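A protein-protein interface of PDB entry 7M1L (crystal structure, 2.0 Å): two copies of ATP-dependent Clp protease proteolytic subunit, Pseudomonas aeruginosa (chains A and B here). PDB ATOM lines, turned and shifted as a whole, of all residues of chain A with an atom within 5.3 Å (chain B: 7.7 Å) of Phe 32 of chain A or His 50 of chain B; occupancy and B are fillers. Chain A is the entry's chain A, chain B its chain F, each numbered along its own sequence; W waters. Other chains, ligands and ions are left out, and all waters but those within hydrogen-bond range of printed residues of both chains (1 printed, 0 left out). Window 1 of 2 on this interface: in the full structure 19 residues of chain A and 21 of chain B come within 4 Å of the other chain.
Of the printed residues of chain B, Val 28 of chain A touches Ser 54 (3.5 Å). Phe 32 of chain A touches just these residues of chain B: Gln 47 (3.7 Å) and His 50 (3.8 Å). Gln 48 of chain A touches none of the printed residues of chain B. Of the printed residues of chain B, Phe 63 of chain A touches His 50 (3.4 Å) and Phe 83 (3.8 Å). His 50 of chain B touches three residues of chain A. Leu 52 of chain B touches none of the printed residues of chain A. Of the printed residues of chain A, Ser 54 of chain B touches Val 28 (3.5 Å) and Lys 30 (2.9 Å). Of the printed residues of chain A, Ile 84 of chain B touches Glu 193 (3.6 Å). Printed residues of chain A within 4 Å of Thr 85 of chain B: Glu 193 (2.8 Å).
Val 28 of chain A touches Ser 54 of chain B. Phe 32 of chain A touches Gln 47 of chain B. Phe 32 of chain A touches His 50 of chain B (CZ to CB, 3.8 Å). O of Thr 34 of chain A touches NZ of Lys 43 of chain B, 3.5 Å away. Thr 34 of chain A touches Met 76 of chain B. Phe 63 of chain A touches His 50 of chain B (CE2 to CE1, 3.4 Å). Phe 63 of chain A touches Phe 83 of chain B. Glu 193 of chain A touches Ile 84 of chain B.
Positions printed for both chains: 45 and 48. Of the 12 pairs that touch across the chains among the printed residues, none has its exchanged pair printed and touching as well.
The backbone NH (N) of Lys 30 of chain A lies within hydrogen-bond range of the backbone carbonyl oxygen (O) of Ala 25 of chain A. O of Val 31 of chain A is in hydrogen-bond range of N of Phe 63 of chain A. N of Val 33 of chain A lies within hydrogen-bond range of O of Phe 63 of chain A, 2.8 Å away. The backbone carbonyl oxygen (O) of Lys 43 of chain B lies close to the side-chain amide nitrogen (NE2) of Gln 47 of chain B, 3.5 Å away. The backbone carbonyl oxygen of His 50 of chain B is in hydrogen-bond range of the side-chain hydroxyl of Ser 54 of chain B, 3.1 Å away.
The backbone carbonyl oxygen (O) of His 50 of chain B is in hydrogen-bond range of the side-chain amino group (NZ) of Lys 30 of chain A (3.0 Å). NZ of Lys 30 of chain A is in hydrogen-bond range of OG of Ser 54 of chain B (2.9 Å). N of Glu 193 of chain A lies within hydrogen-bond range of O of Phe 83 of chain B. The backbone NH (N) of Thr 85 of chain B is in hydrogen-bond range of the side-chain carboxylate (OE2) of Glu 193 of chain A (2.8 Å).
Of the 11 printed residues of chain A, 6 touch a printed residue of chain B. Hydrophobic or aromatic side chains of chain A that line the printed part of chain B: Val 28, Phe 32 and Phe 63. Of the 24 printed residues of chain B, 8 touch a printed residue of chain A. Hydrophobic or aromatic side chains of chain B that line the printed part of chain A: His 50, Met 76 and Phe 83. Among the printed residues, 12 pairs touch across the chains. Among the printed residues, no Asp or Glu carboxylate lies within 4 Å of a Lys or Arg side-chain nitrogen of the other chain.
Water W1 bridges the side-chain carboxylate of Glu 193 of chain A (2.8 Å) and the backbone carbonyl oxygen of Ala 53 of chain B (3.3 Å).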
ATOM      1  N   ALA A  25      15.367   6.243  26.729  1.00  0.00           N
ATOM      2  CA  ALA A  25      14.978   5.356  25.634  1.00  0.00           C
ATOM      3  C   ALA A  25      13.692   4.609  25.968  1.00  0.00           C
ATOM      4  O   ALA A  25      12.817   4.437  25.110  1.00  0.00           O
ATOM      5  CB  ALA A  25      16.111   4.377  25.323  1.00  0.00           C
ATOM      6  N   VAL A  28      10.665   6.719  25.364  1.00  0.00           N
ATOM      7  CA  VAL A  28      10.297   6.877  23.961  1.00  0.00           C
ATOM      8  C   VAL A  28      10.149   5.533  23.268  1.00  0.00           C
ATOM      9  O   VAL A  28      10.054   5.485  22.041  1.00  0.00           O
ATOM     10  CB  VAL A  28      11.295   7.769  23.203  1.00  0.00           C
ATOM     11  CG1 VAL A  28      11.370   9.118  23.868  1.00  0.00           C
ATOM     12  CG2 VAL A  28      12.659   7.104  23.128  1.00  0.00           C
ATOM     13  N   LYS A  30      12.112   2.903  22.688  1.00  0.00           N
ATOM     14  CA  LYS A  30      13.160   2.469  21.779  1.00  0.00           C
ATOM     15  C   LYS A  30      14.111   1.586  22.566  1.00  0.00           C
ATOM     16  O   LYS A  30      14.527   1.953  23.671  1.00  0.00           O
ATOM     17  CB  LYS A  30      13.879   3.659  21.164  1.00  0.00           C
ATOM     18  CG  LYS A  30      12.979   4.457  20.259  1.00  0.00           C
ATOM     19  CD  LYS A  30      13.696   5.654  19.633  1.00  0.00           C
ATOM     20  CE  LYS A  30      12.799   6.315  18.612  1.00  0.00           C
ATOM     21  NZ  LYS A  30      13.479   7.455  17.910  1.00  0.00           N
ATOM     22  N   VAL A  31      14.457   0.437  21.984  1.00  0.00           N
ATOM     23  CA  VAL A  31      15.356  -0.547  22.577  1.00  0.00           C
ATOM     24  C   VAL A  31      16.484  -0.763  21.584  1.00  0.00           C
ATOM     25  O   VAL A  31      16.229  -1.045  20.403  1.00  0.00           O
ATOM     26  CB  VAL A  31      14.617  -1.881  22.853  1.00  0.00           C
ATOM     27  CG1 VAL A  31      15.550  -2.931  23.431  1.00  0.00           C
ATOM     28  CG2 VAL A  31      13.426  -1.661  23.793  1.00  0.00           C
ATOM     29  N   PHE A  32      17.709  -0.737  22.075  1.00  0.00           N
ATOM     30  CA  PHE A  32      18.905  -0.868  21.258  1.00  0.00           C
ATOM     31  C   PHE A  32      19.573  -2.194  21.571  1.00  0.00           C
ATOM     32  O   PHE A  32      19.874  -2.483  22.734  1.00  0.00           O
ATOM     33  CB  PHE A  32      19.832   0.323  21.530  1.00  0.00           C
ATOM     34  CG  PHE A  32      19.222   1.619  21.079  1.00  0.00           C
ATOM     35  CD1 PHE A  32      18.403   2.347  21.925  1.00  0.00           C
ATOM     36  CD2 PHE A  32      19.381   2.043  19.765  1.00  0.00           C
ATOM     37  CE1 PHE A  32      17.795   3.509  21.482  1.00  0.00           C
ATOM     38  CE2 PHE A  32      18.778   3.205  19.312  1.00  0.00           C
ATOM     39  CZ  PHE A  32      17.973   3.927  20.163  1.00  0.00           C
ATOM     40  N   VAL A  33      19.776  -2.998  20.526  1.00  0.00           N
ATOM     41  CA  VAL A  33      20.500  -4.259  20.570  1.00  0.00           C
ATOM     42  C   VAL A  33      21.762  -4.043  19.745  1.00  0.00           C
ATOM     43  O   VAL A  33      21.754  -4.169  18.516  1.00  0.00           O
ATOM     44  CB  VAL A  33      19.651  -5.422  20.018  1.00  0.00           C
ATOM     45  CG1 VAL A  33      20.493  -6.694  19.922  1.00  0.00           C
ATOM     46  CG2 VAL A  33      18.439  -5.651  20.917  1.00  0.00           C
ATOM     47  N   THR A  34      22.843  -3.671  20.409  1.00  0.00           N
ATOM     48  CA  THR A  34      24.067  -3.250  19.750  1.00  0.00           C
ATOM     49  C   THR A  34      25.200  -4.142  20.229  1.00  0.00           C
ATOM     50  O   THR A  34      25.413  -4.277  21.442  1.00  0.00           O
ATOM     51  CB  THR A  34      24.390  -1.783  20.084  1.00  0.00           C
ATOM     52  OG1 THR A  34      23.239  -0.958  19.858  1.00  0.00           O
ATOM     53  CG2 THR A  34      25.548  -1.281  19.236  1.00  0.00           C
ATOM     54  N   VAL A  45      17.400  -6.510  27.924  1.00  0.00           N
ATOM     55  CA  VAL A  45      16.410  -6.316  26.865  1.00  0.00           C
ATOM     56  C   VAL A  45      15.079  -6.947  27.254  1.00  0.00           C
ATOM     57  O   VAL A  45      14.012  -6.359  27.043  1.00  0.00           O
ATOM     58  CB  VAL A  45      16.918  -6.860  25.518  1.00  0.00           C
ATOM     59  CG1 VAL A  45      15.773  -6.805  24.476  1.00  0.00           C
ATOM     60  CG2 VAL A  45      18.131  -6.060  25.079  1.00  0.00           C
ATOM     61  N   GLN A  48      13.379  -4.639  29.632  1.00  0.00           N
ATOM     62  CA  GLN A  48      12.882  -3.461  28.931  1.00  0.00           C
ATOM     63  C   GLN A  48      11.584  -3.749  28.209  1.00  0.00           C
ATOM     64  O   GLN A  48      10.651  -2.936  28.234  1.00  0.00           O
ATOM     65  CB  GLN A  48      13.921  -2.944  27.942  1.00  0.00           C
ATOM     66  CG  GLN A  48      15.139  -2.346  28.589  1.00  0.00           C
ATOM     67  CD  GLN A  48      16.209  -2.004  27.577  1.00  0.00           C
ATOM     68  OE1 GLN A  48      17.223  -2.693  27.476  1.00  0.00           O
ATOM     69  NE2 GLN A  48      15.952  -0.975  26.766  1.00  0.00           N
ATOM     70  N   PHE A  63      16.282  -1.527  17.480  1.00  0.00           N
ATOM     71  CA  PHE A  63      17.378  -1.269  16.557  1.00  0.00           C
ATOM     72  C   PHE A  63      18.433  -2.327  16.805  1.00  0.00           C
ATOM     73  O   PHE A  63      18.981  -2.408  17.909  1.00  0.00           O
ATOM     74  CB  PHE A  63      17.933   0.144  16.760  1.00  0.00           C
ATOM     75  CG  PHE A  63      16.908   1.220  16.547  1.00  0.00           C
ATOM     76  CD1 PHE A  63      16.111   1.650  17.591  1.00  0.00           C
ATOM     77  CD2 PHE A  63      16.705   1.766  15.280  1.00  0.00           C
ATOM     78  CE1 PHE A  63      15.140   2.616  17.397  1.00  0.00           C
ATOM     79  CE2 PHE A  63      15.744   2.749  15.088  1.00  0.00           C
ATOM     80  CZ  PHE A  63      14.954   3.162  16.151  1.00  0.00           C
ATOM     81  N   GLU A 193      13.261   6.999   9.038  1.00  0.00           N
ATOM     82  CA  GLU A 193      12.175   6.530   9.889  1.00  0.00           C
ATOM     83  C   GLU A 193      10.818   6.880   9.296  1.00  0.00           C
ATOM     84  O   GLU A 193       9.826   6.212   9.600  1.00  0.00           O
ATOM     85  CB  GLU A 193      12.300   7.130  11.303  1.00  0.00           C
ATOM     86  CG  GLU A 193      12.224   8.668  11.370  1.00  0.00           C
ATOM     87  CD  GLU A 193      12.527   9.196  12.780  1.00  0.00           C
ATOM     88  OE1 GLU A 193      12.729   8.367  13.692  1.00  0.00           O
ATOM     89  OE2 GLU A 193      12.502  10.430  12.985  1.00  0.00           O
ATOM     90  N   LEU B  26      20.977  17.050  26.351  1.00  0.00           N
ATOM     91  CA  LEU B  26      19.752  16.594  25.707  1.00  0.00           C
ATOM     92  C   LEU B  26      18.667  17.662  25.765  1.00  0.00           C
ATOM     93  O   LEU B  26      17.974  17.913  24.770  1.00  0.00           O
ATOM     94  CB  LEU B  26      19.272  15.312  26.387  1.00  0.00           C
ATOM     95  CG  LEU B  26      19.898  13.994  25.946  1.00  0.00           C
ATOM     96  CD1 LEU B  26      19.350  12.845  26.810  1.00  0.00           C
ATOM     97  CD2 LEU B  26      19.641  13.740  24.477  1.00  0.00           C
ATOM     98  N   LYS B  43      27.522   4.290  20.488  1.00  0.00           N
ATOM     99  CA  LYS B  43      26.335   3.855  21.214  1.00  0.00           C
ATOM    100  C   LYS B  43      25.629   5.039  21.857  1.00  0.00           C
ATOM    101  O   LYS B  43      24.411   5.194  21.726  1.00  0.00           O
ATOM    102  CB  LYS B  43      26.671   2.814  22.282  1.00  0.00           C
ATOM    103  CG  LYS B  43      27.039   1.449  21.769  1.00  0.00           C
ATOM    104  CD  LYS B  43      27.063   0.445  22.939  1.00  0.00           C
ATOM    105  CE  LYS B  43      27.234  -0.986  22.438  1.00  0.00           C
ATOM    106  NZ  LYS B  43      27.098  -1.992  23.533  1.00  0.00           N
ATOM    107  N   ASP B  44      26.387   5.904  22.539  1.00  0.00           N
ATOM    108  CA  ASP B  44      25.777   7.040  23.225  1.00  0.00           C
ATOM    109  C   ASP B  44      25.167   8.026  22.236  1.00  0.00           C
ATOM    110  O   ASP B  44      24.058   8.532  22.450  1.00  0.00           O
ATOM    111  CB  ASP B  44      26.811   7.773  24.086  1.00  0.00           C
ATOM    112  CG  ASP B  44      27.271   6.967  25.289  1.00  0.00           C
ATOM    113  OD1 ASP B  44      26.643   5.923  25.600  1.00  0.00           O
ATOM    114  OD2 ASP B  44      28.255   7.407  25.938  1.00  0.00           O
ATOM    115  N   VAL B  45      25.906   8.365  21.173  1.00  0.00           N
ATOM    116  CA  VAL B  45      25.416   9.381  20.242  1.00  0.00           C
ATOM    117  C   VAL B  45      24.170   8.893  19.521  1.00  0.00           C
ATOM    118  O   VAL B  45      23.227   9.663  19.302  1.00  0.00           O
ATOM    119  CB  VAL B  45      26.513   9.796  19.241  1.00  0.00           C
ATOM    120  CG1 VAL B  45      25.931  10.706  18.140  1.00  0.00           C
ATOM    121  CG2 VAL B  45      27.635  10.522  19.995  1.00  0.00           C
ATOM    122  N   VAL B  46      24.154   7.627  19.109  1.00  0.00           N
ATOM    123  CA  VAL B  46      22.985   7.111  18.395  1.00  0.00           C
ATOM    124  C   VAL B  46      21.745   7.192  19.275  1.00  0.00           C
ATOM    125  O   VAL B  46      20.674   7.616  18.827  1.00  0.00           O
ATOM    126  CB  VAL B  46      23.239   5.678  17.889  1.00  0.00           C
ATOM    127  CG1 VAL B  46      21.935   5.045  17.461  1.00  0.00           C
ATOM    128  CG2 VAL B  46      24.232   5.676  16.726  1.00  0.00           C
ATOM    129  N   GLN B  47      21.865   6.795  20.541  1.00  0.00           N
ATOM    130  CA  GLN B  47      20.724   6.889  21.443  1.00  0.00           C
ATOM    131  C   GLN B  47      20.271   8.332  21.653  1.00  0.00           C
ATOM    132  O   GLN B  47      19.064   8.627  21.640  1.00  0.00           O
ATOM    133  CB  GLN B  47      21.095   6.218  22.761  1.00  0.00           C
ATOM    134  CG  GLN B  47      21.214   4.696  22.687  1.00  0.00           C
ATOM    135  CD  GLN B  47      21.449   4.113  24.070  1.00  0.00           C
ATOM    136  OE1 GLN B  47      20.523   4.015  24.854  1.00  0.00           O
ATOM    137  NE2 GLN B  47      22.671   3.671  24.347  1.00  0.00           N
ATOM    138  N   GLN B  48      21.216   9.244  21.876  1.00  0.00           N
ATOM    139  CA  GLN B  48      20.857  10.649  22.021  1.00  0.00           C
ATOM    140  C   GLN B  48      20.076  11.151  20.810  1.00  0.00           C
ATOM    141  O   GLN B  48      19.053  11.832  20.946  1.00  0.00           O
ATOM    142  CB  GLN B  48      22.119  11.494  22.189  1.00  0.00           C
ATOM    143  CG  GLN B  48      22.873  11.361  23.467  1.00  0.00           C
ATOM    144  CD  GLN B  48      24.211  12.113  23.416  1.00  0.00           C
ATOM    145  OE1 GLN B  48      25.273  11.507  23.358  1.00  0.00           O
ATOM    146  NE2 GLN B  48      24.143  13.433  23.332  1.00  0.00           N
ATOM    147  N   LEU B  49      20.564  10.857  19.608  1.00  0.00           N
ATOM    148  CA  LEU B  49      19.859  11.320  18.412  1.00  0.00           C
ATOM    149  C   LEU B  49      18.430  10.790  18.365  1.00  0.00           C
ATOM    150  O   LEU B  49      17.484  11.552  18.114  1.00  0.00           O
ATOM    151  CB  LEU B  49      20.633  10.892  17.162  1.00  0.00           C
ATOM    152  CG  LEU B  49      21.953  11.640  16.944  1.00  0.00           C
ATOM    153  CD1 LEU B  49      22.754  10.946  15.859  1.00  0.00           C
ATOM    154  CD2 LEU B  49      21.676  13.097  16.587  1.00  0.00           C
ATOM    155  N   HIS B  50      18.249   9.495  18.663  1.00  0.00           N
ATOM    156  CA  HIS B  50      16.912   8.896  18.620  1.00  0.00           C
ATOM    157  C   HIS B  50      16.014   9.449  19.714  1.00  0.00           C
ATOM    158  O   HIS B  50      14.811   9.630  19.496  1.00  0.00           O
ATOM    159  CB  HIS B  50      16.997   7.367  18.741  1.00  0.00           C
ATOM    160  CG  HIS B  50      17.301   6.696  17.444  1.00  0.00           C
ATOM    161  ND1 HIS B  50      16.346   6.516  16.466  1.00  0.00           N
ATOM    162  CD2 HIS B  50      18.463   6.225  16.932  1.00  0.00           C
ATOM    163  CE1 HIS B  50      16.901   5.938  15.416  1.00  0.00           C
ATOM    164  NE2 HIS B  50      18.187   5.767  15.663  1.00  0.00           N
ATOM    165  N   ILE B  51      16.572   9.688  20.906  1.00  0.00           N
ATOM    166  CA  ILE B  51      15.790  10.287  21.982  1.00  0.00           C
ATOM    167  C   ILE B  51      15.321  11.674  21.565  1.00  0.00           C
ATOM    168  O   ILE B  51      14.145  12.027  21.702  1.00  0.00           O
ATOM    169  CB  ILE B  51      16.621  10.341  23.283  1.00  0.00           C
ATOM    170  CG1 ILE B  51      16.828   8.932  23.860  1.00  0.00           C
ATOM    171  CG2 ILE B  51      15.929  11.241  24.296  1.00  0.00           C
ATOM    172  CD1 ILE B  51      18.007   8.820  24.797  1.00  0.00           C
ATOM    173  N   LEU B  52      16.249  12.490  21.057  1.00  0.00           N
ATOM    174  CA  LEU B  52      15.895  13.841  20.620  1.00  0.00           C
ATOM    175  C   LEU B  52      14.863  13.818  19.506  1.00  0.00           C
ATOM    176  O   LEU B  52      13.947  14.653  19.477  1.00  0.00           O
ATOM    177  CB  LEU B  52      17.151  14.574  20.144  1.00  0.00           C
ATOM    178  CG  LEU B  52      18.182  14.873  21.215  1.00  0.00           C
ATOM    179  CD1 LEU B  52      19.462  15.427  20.635  1.00  0.00           C
ATOM    180  CD2 LEU B  52      17.568  15.855  22.235  1.00  0.00           C
ATOM    181  N   ALA B  53      15.001  12.875  18.564  1.00  0.00           N
ATOM    182  CA  ALA B  53      14.031  12.780  17.473  1.00  0.00           C
ATOM    183  C   ALA B  53      12.645  12.417  17.987  1.00  0.00           C
ATOM    184  O   ALA B  53      11.640  12.934  17.493  1.00  0.00           O
ATOM    185  CB  ALA B  53      14.490  11.750  16.438  1.00  0.00           C
ATOM    186  N   SER B  54      12.563  11.562  19.007  1.00  0.00           N
ATOM    187  CA  SER B  54      11.254  11.211  19.550  1.00  0.00           C
ATOM    188  C   SER B  54      10.634  12.379  20.304  1.00  0.00           C
ATOM    189  O   SER B  54       9.406  12.466  20.410  1.00  0.00           O
ATOM    190  CB  SER B  54      11.365   9.996  20.473  1.00  0.00           C
ATOM    191  OG  SER B  54      11.824   8.864  19.761  1.00  0.00           O
ATOM    192  N   ILE B  55      11.467  13.262  20.863  1.00  0.00           N
ATOM    193  CA  ILE B  55      10.957  14.380  21.648  1.00  0.00           C
ATOM    194  C   ILE B  55      10.381  15.455  20.737  1.00  0.00           C
ATOM    195  O   ILE B  55       9.318  16.017  21.015  1.00  0.00           O
ATOM    196  CB  ILE B  55      12.066  14.934  22.562  1.00  0.00           C
ATOM    197  CG1 ILE B  55      12.414  13.908  23.649  1.00  0.00           C
ATOM    198  CG2 ILE B  55      11.645  16.253  23.186  1.00  0.00           C
ATOM    199  CD1 ILE B  55      13.617  14.311  24.524  1.00  0.00           C
ATOM    200  N   SER B  56      11.062  15.764  19.640  1.00  0.00           N
ATOM    201  CA  SER B  56      10.522  16.757  18.722  1.00  0.00           C
ATOM    202  C   SER B  56      11.255  16.686  17.392  1.00  0.00           C
ATOM    203  O   SER B  56      12.294  16.039  17.258  1.00  0.00           O
ATOM    204  CB  SER B  56      10.618  18.175  19.307  1.00  0.00           C
ATOM    205  OG  SER B  56      11.891  18.749  19.074  1.00  0.00           O
ATOM    206  N   ILE B  60      18.784  19.696  15.643  1.00  0.00           N
ATOM    207  CA  ILE B  60      19.770  19.184  16.592  1.00  0.00           C
ATOM    208  C   ILE B  60      21.118  19.743  16.183  1.00  0.00           C
ATOM    209  O   ILE B  60      21.475  19.693  14.995  1.00  0.00           O
ATOM    210  CB  ILE B  60      19.817  17.643  16.608  1.00  0.00           C
ATOM    211  CG1 ILE B  60      18.488  17.086  17.068  1.00  0.00           C
ATOM    212  CG2 ILE B  60      20.971  17.139  17.473  1.00  0.00           C
ATOM    213  CD1 ILE B  60      18.338  15.576  16.806  1.00  0.00           C
ATOM    214  N   MET B  76      27.655   4.042  12.134  1.00  0.00           N
ATOM    215  CA  MET B  76      26.463   4.017  12.972  1.00  0.00           C
ATOM    216  C   MET B  76      25.914   5.413  13.207  1.00  0.00           C
ATOM    217  O   MET B  76      24.693   5.624  13.204  1.00  0.00           O
ATOM    218  CB  MET B  76      26.777   3.362  14.320  1.00  0.00           C
ATOM    219  CG  MET B  76      26.763   1.867  14.369  1.00  0.00           C
ATOM    220  SD  MET B  76      27.086   1.366  16.084  1.00  0.00           S
ATOM    221  CE  MET B  76      25.435   1.544  16.771  1.00  0.00           C
ATOM    222  N   ASP B  79      24.525   6.728   9.889  1.00  0.00           N
ATOM    223  CA  ASP B  79      23.233   6.110   9.598  1.00  0.00           C
ATOM    224  C   ASP B  79      22.125   6.705  10.448  1.00  0.00           C
ATOM    225  O   ASP B  79      21.008   6.914   9.960  1.00  0.00           O
ATOM    226  CB  ASP B  79      23.316   4.607   9.834  1.00  0.00           C
ATOM    227  CG  ASP B  79      24.031   3.881   8.718  1.00  0.00           C
ATOM    228  OD1 ASP B  79      24.027   4.386   7.565  1.00  0.00           O
ATOM    229  OD2 ASP B  79      24.575   2.789   8.985  1.00  0.00           O
ATOM    230  N   ALA B  80      22.412   6.981  11.732  1.00  0.00           N
ATOM    231  CA  ALA B  80      21.390   7.533  12.616  1.00  0.00           C
ATOM    232  C   ALA B  80      21.028   8.954  12.227  1.00  0.00           C
ATOM    233  O   ALA B  80      19.852   9.334  12.269  1.00  0.00           O
ATOM    234  CB  ALA B  80      21.856   7.480  14.077  1.00  0.00           C
ATOM    235  N   ILE B  81      22.028   9.771  11.885  1.00  0.00           N
ATOM    236  CA  ILE B  81      21.742  11.127  11.425  1.00  0.00           C
ATOM    237  C   ILE B  81      20.794  11.093  10.240  1.00  0.00           C
ATOM    238  O   ILE B  81      19.823  11.854  10.182  1.00  0.00           O
ATOM    239  CB  ILE B  81      23.048  11.861  11.065  1.00  0.00           C
ATOM    240  CG1 ILE B  81      23.867  12.135  12.322  1.00  0.00           C
ATOM    241  CG2 ILE B  81      22.749  13.185  10.307  1.00  0.00           C
ATOM    242  CD1 ILE B  81      25.276  12.592  12.021  1.00  0.00           C
ATOM    243  N   PHE B  83      18.756   8.696   9.380  1.00  0.00           N
ATOM    244  CA  PHE B  83      17.504   7.990   9.661  1.00  0.00           C
ATOM    245  C   PHE B  83      16.478   8.904  10.330  1.00  0.00           C
ATOM    246  O   PHE B  83      15.287   8.855   9.995  1.00  0.00           O
ATOM    247  CB  PHE B  83      17.824   6.755  10.537  1.00  0.00           C
ATOM    248  CG  PHE B  83      16.658   5.809  10.729  1.00  0.00           C
ATOM    249  CD1 PHE B  83      16.307   4.921   9.735  1.00  0.00           C
ATOM    250  CD2 PHE B  83      15.923   5.809  11.904  1.00  0.00           C
ATOM    251  CE1 PHE B  83      15.241   4.082   9.889  1.00  0.00           C
ATOM    252  CE2 PHE B  83      14.859   4.949  12.064  1.00  0.00           C
ATOM    253  CZ  PHE B  83      14.516   4.105  11.063  1.00  0.00           C
ATOM    254  N   ILE B  84      16.913   9.744  11.292  1.00  0.00           N
ATOM    255  CA  ILE B  84      15.963  10.514  12.088  1.00  0.00           C
ATOM    256  C   ILE B  84      15.404  11.678  11.277  1.00  0.00           C
ATOM    257  O   ILE B  84      15.998  12.147  10.312  1.00  0.00           O
ATOM    258  CB  ILE B  84      16.593  11.015  13.402  1.00  0.00           C
ATOM    259  CG1 ILE B  84      17.732  11.999  13.103  1.00  0.00           C
ATOM    260  CG2 ILE B  84      17.087   9.832  14.246  1.00  0.00           C
ATOM    261  CD1 ILE B  84      18.301  12.655  14.343  1.00  0.00           C
ATOM    262  N   THR B  85      14.263  12.180  11.724  1.00  0.00           N
ATOM    263  CA  THR B  85      13.580  13.264  11.039  1.00  0.00           C
ATOM    264  C   THR B  85      14.191  14.641  11.300  1.00  0.00           C
ATOM    265  O   THR B  85      14.240  15.459  10.373  1.00  0.00           O
ATOM    266  CB  THR B  85      12.106  13.281  11.441  1.00  0.00           C
ATOM    267  OG1 THR B  85      11.455  12.098  10.952  1.00  0.00           O
ATOM    268  CG2 THR B  85      11.400  14.521  10.870  1.00  0.00           C
ATOM    269  N   PRO B  86      14.608  14.974  12.524  1.00  0.00           N
ATOM    270  CA  PRO B  86      15.190  16.313  12.746  1.00  0.00           C
ATOM    271  C   PRO B  86      16.436  16.526  11.898  1.00  0.00           C
ATOM    272  O   PRO B  86      17.280  15.635  11.770  1.00  0.00           O
ATOM    273  CB  PRO B  86      15.533  16.321  14.245  1.00  0.00           C
ATOM    274  CG  PRO B  86      14.665  15.222  14.847  1.00  0.00           C
ATOM    275  CD  PRO B  86      14.492  14.187  13.770  1.00  0.00           C
HETATM  276  O   HOH W   1      10.616  11.506  14.711  1.00  0.00           O
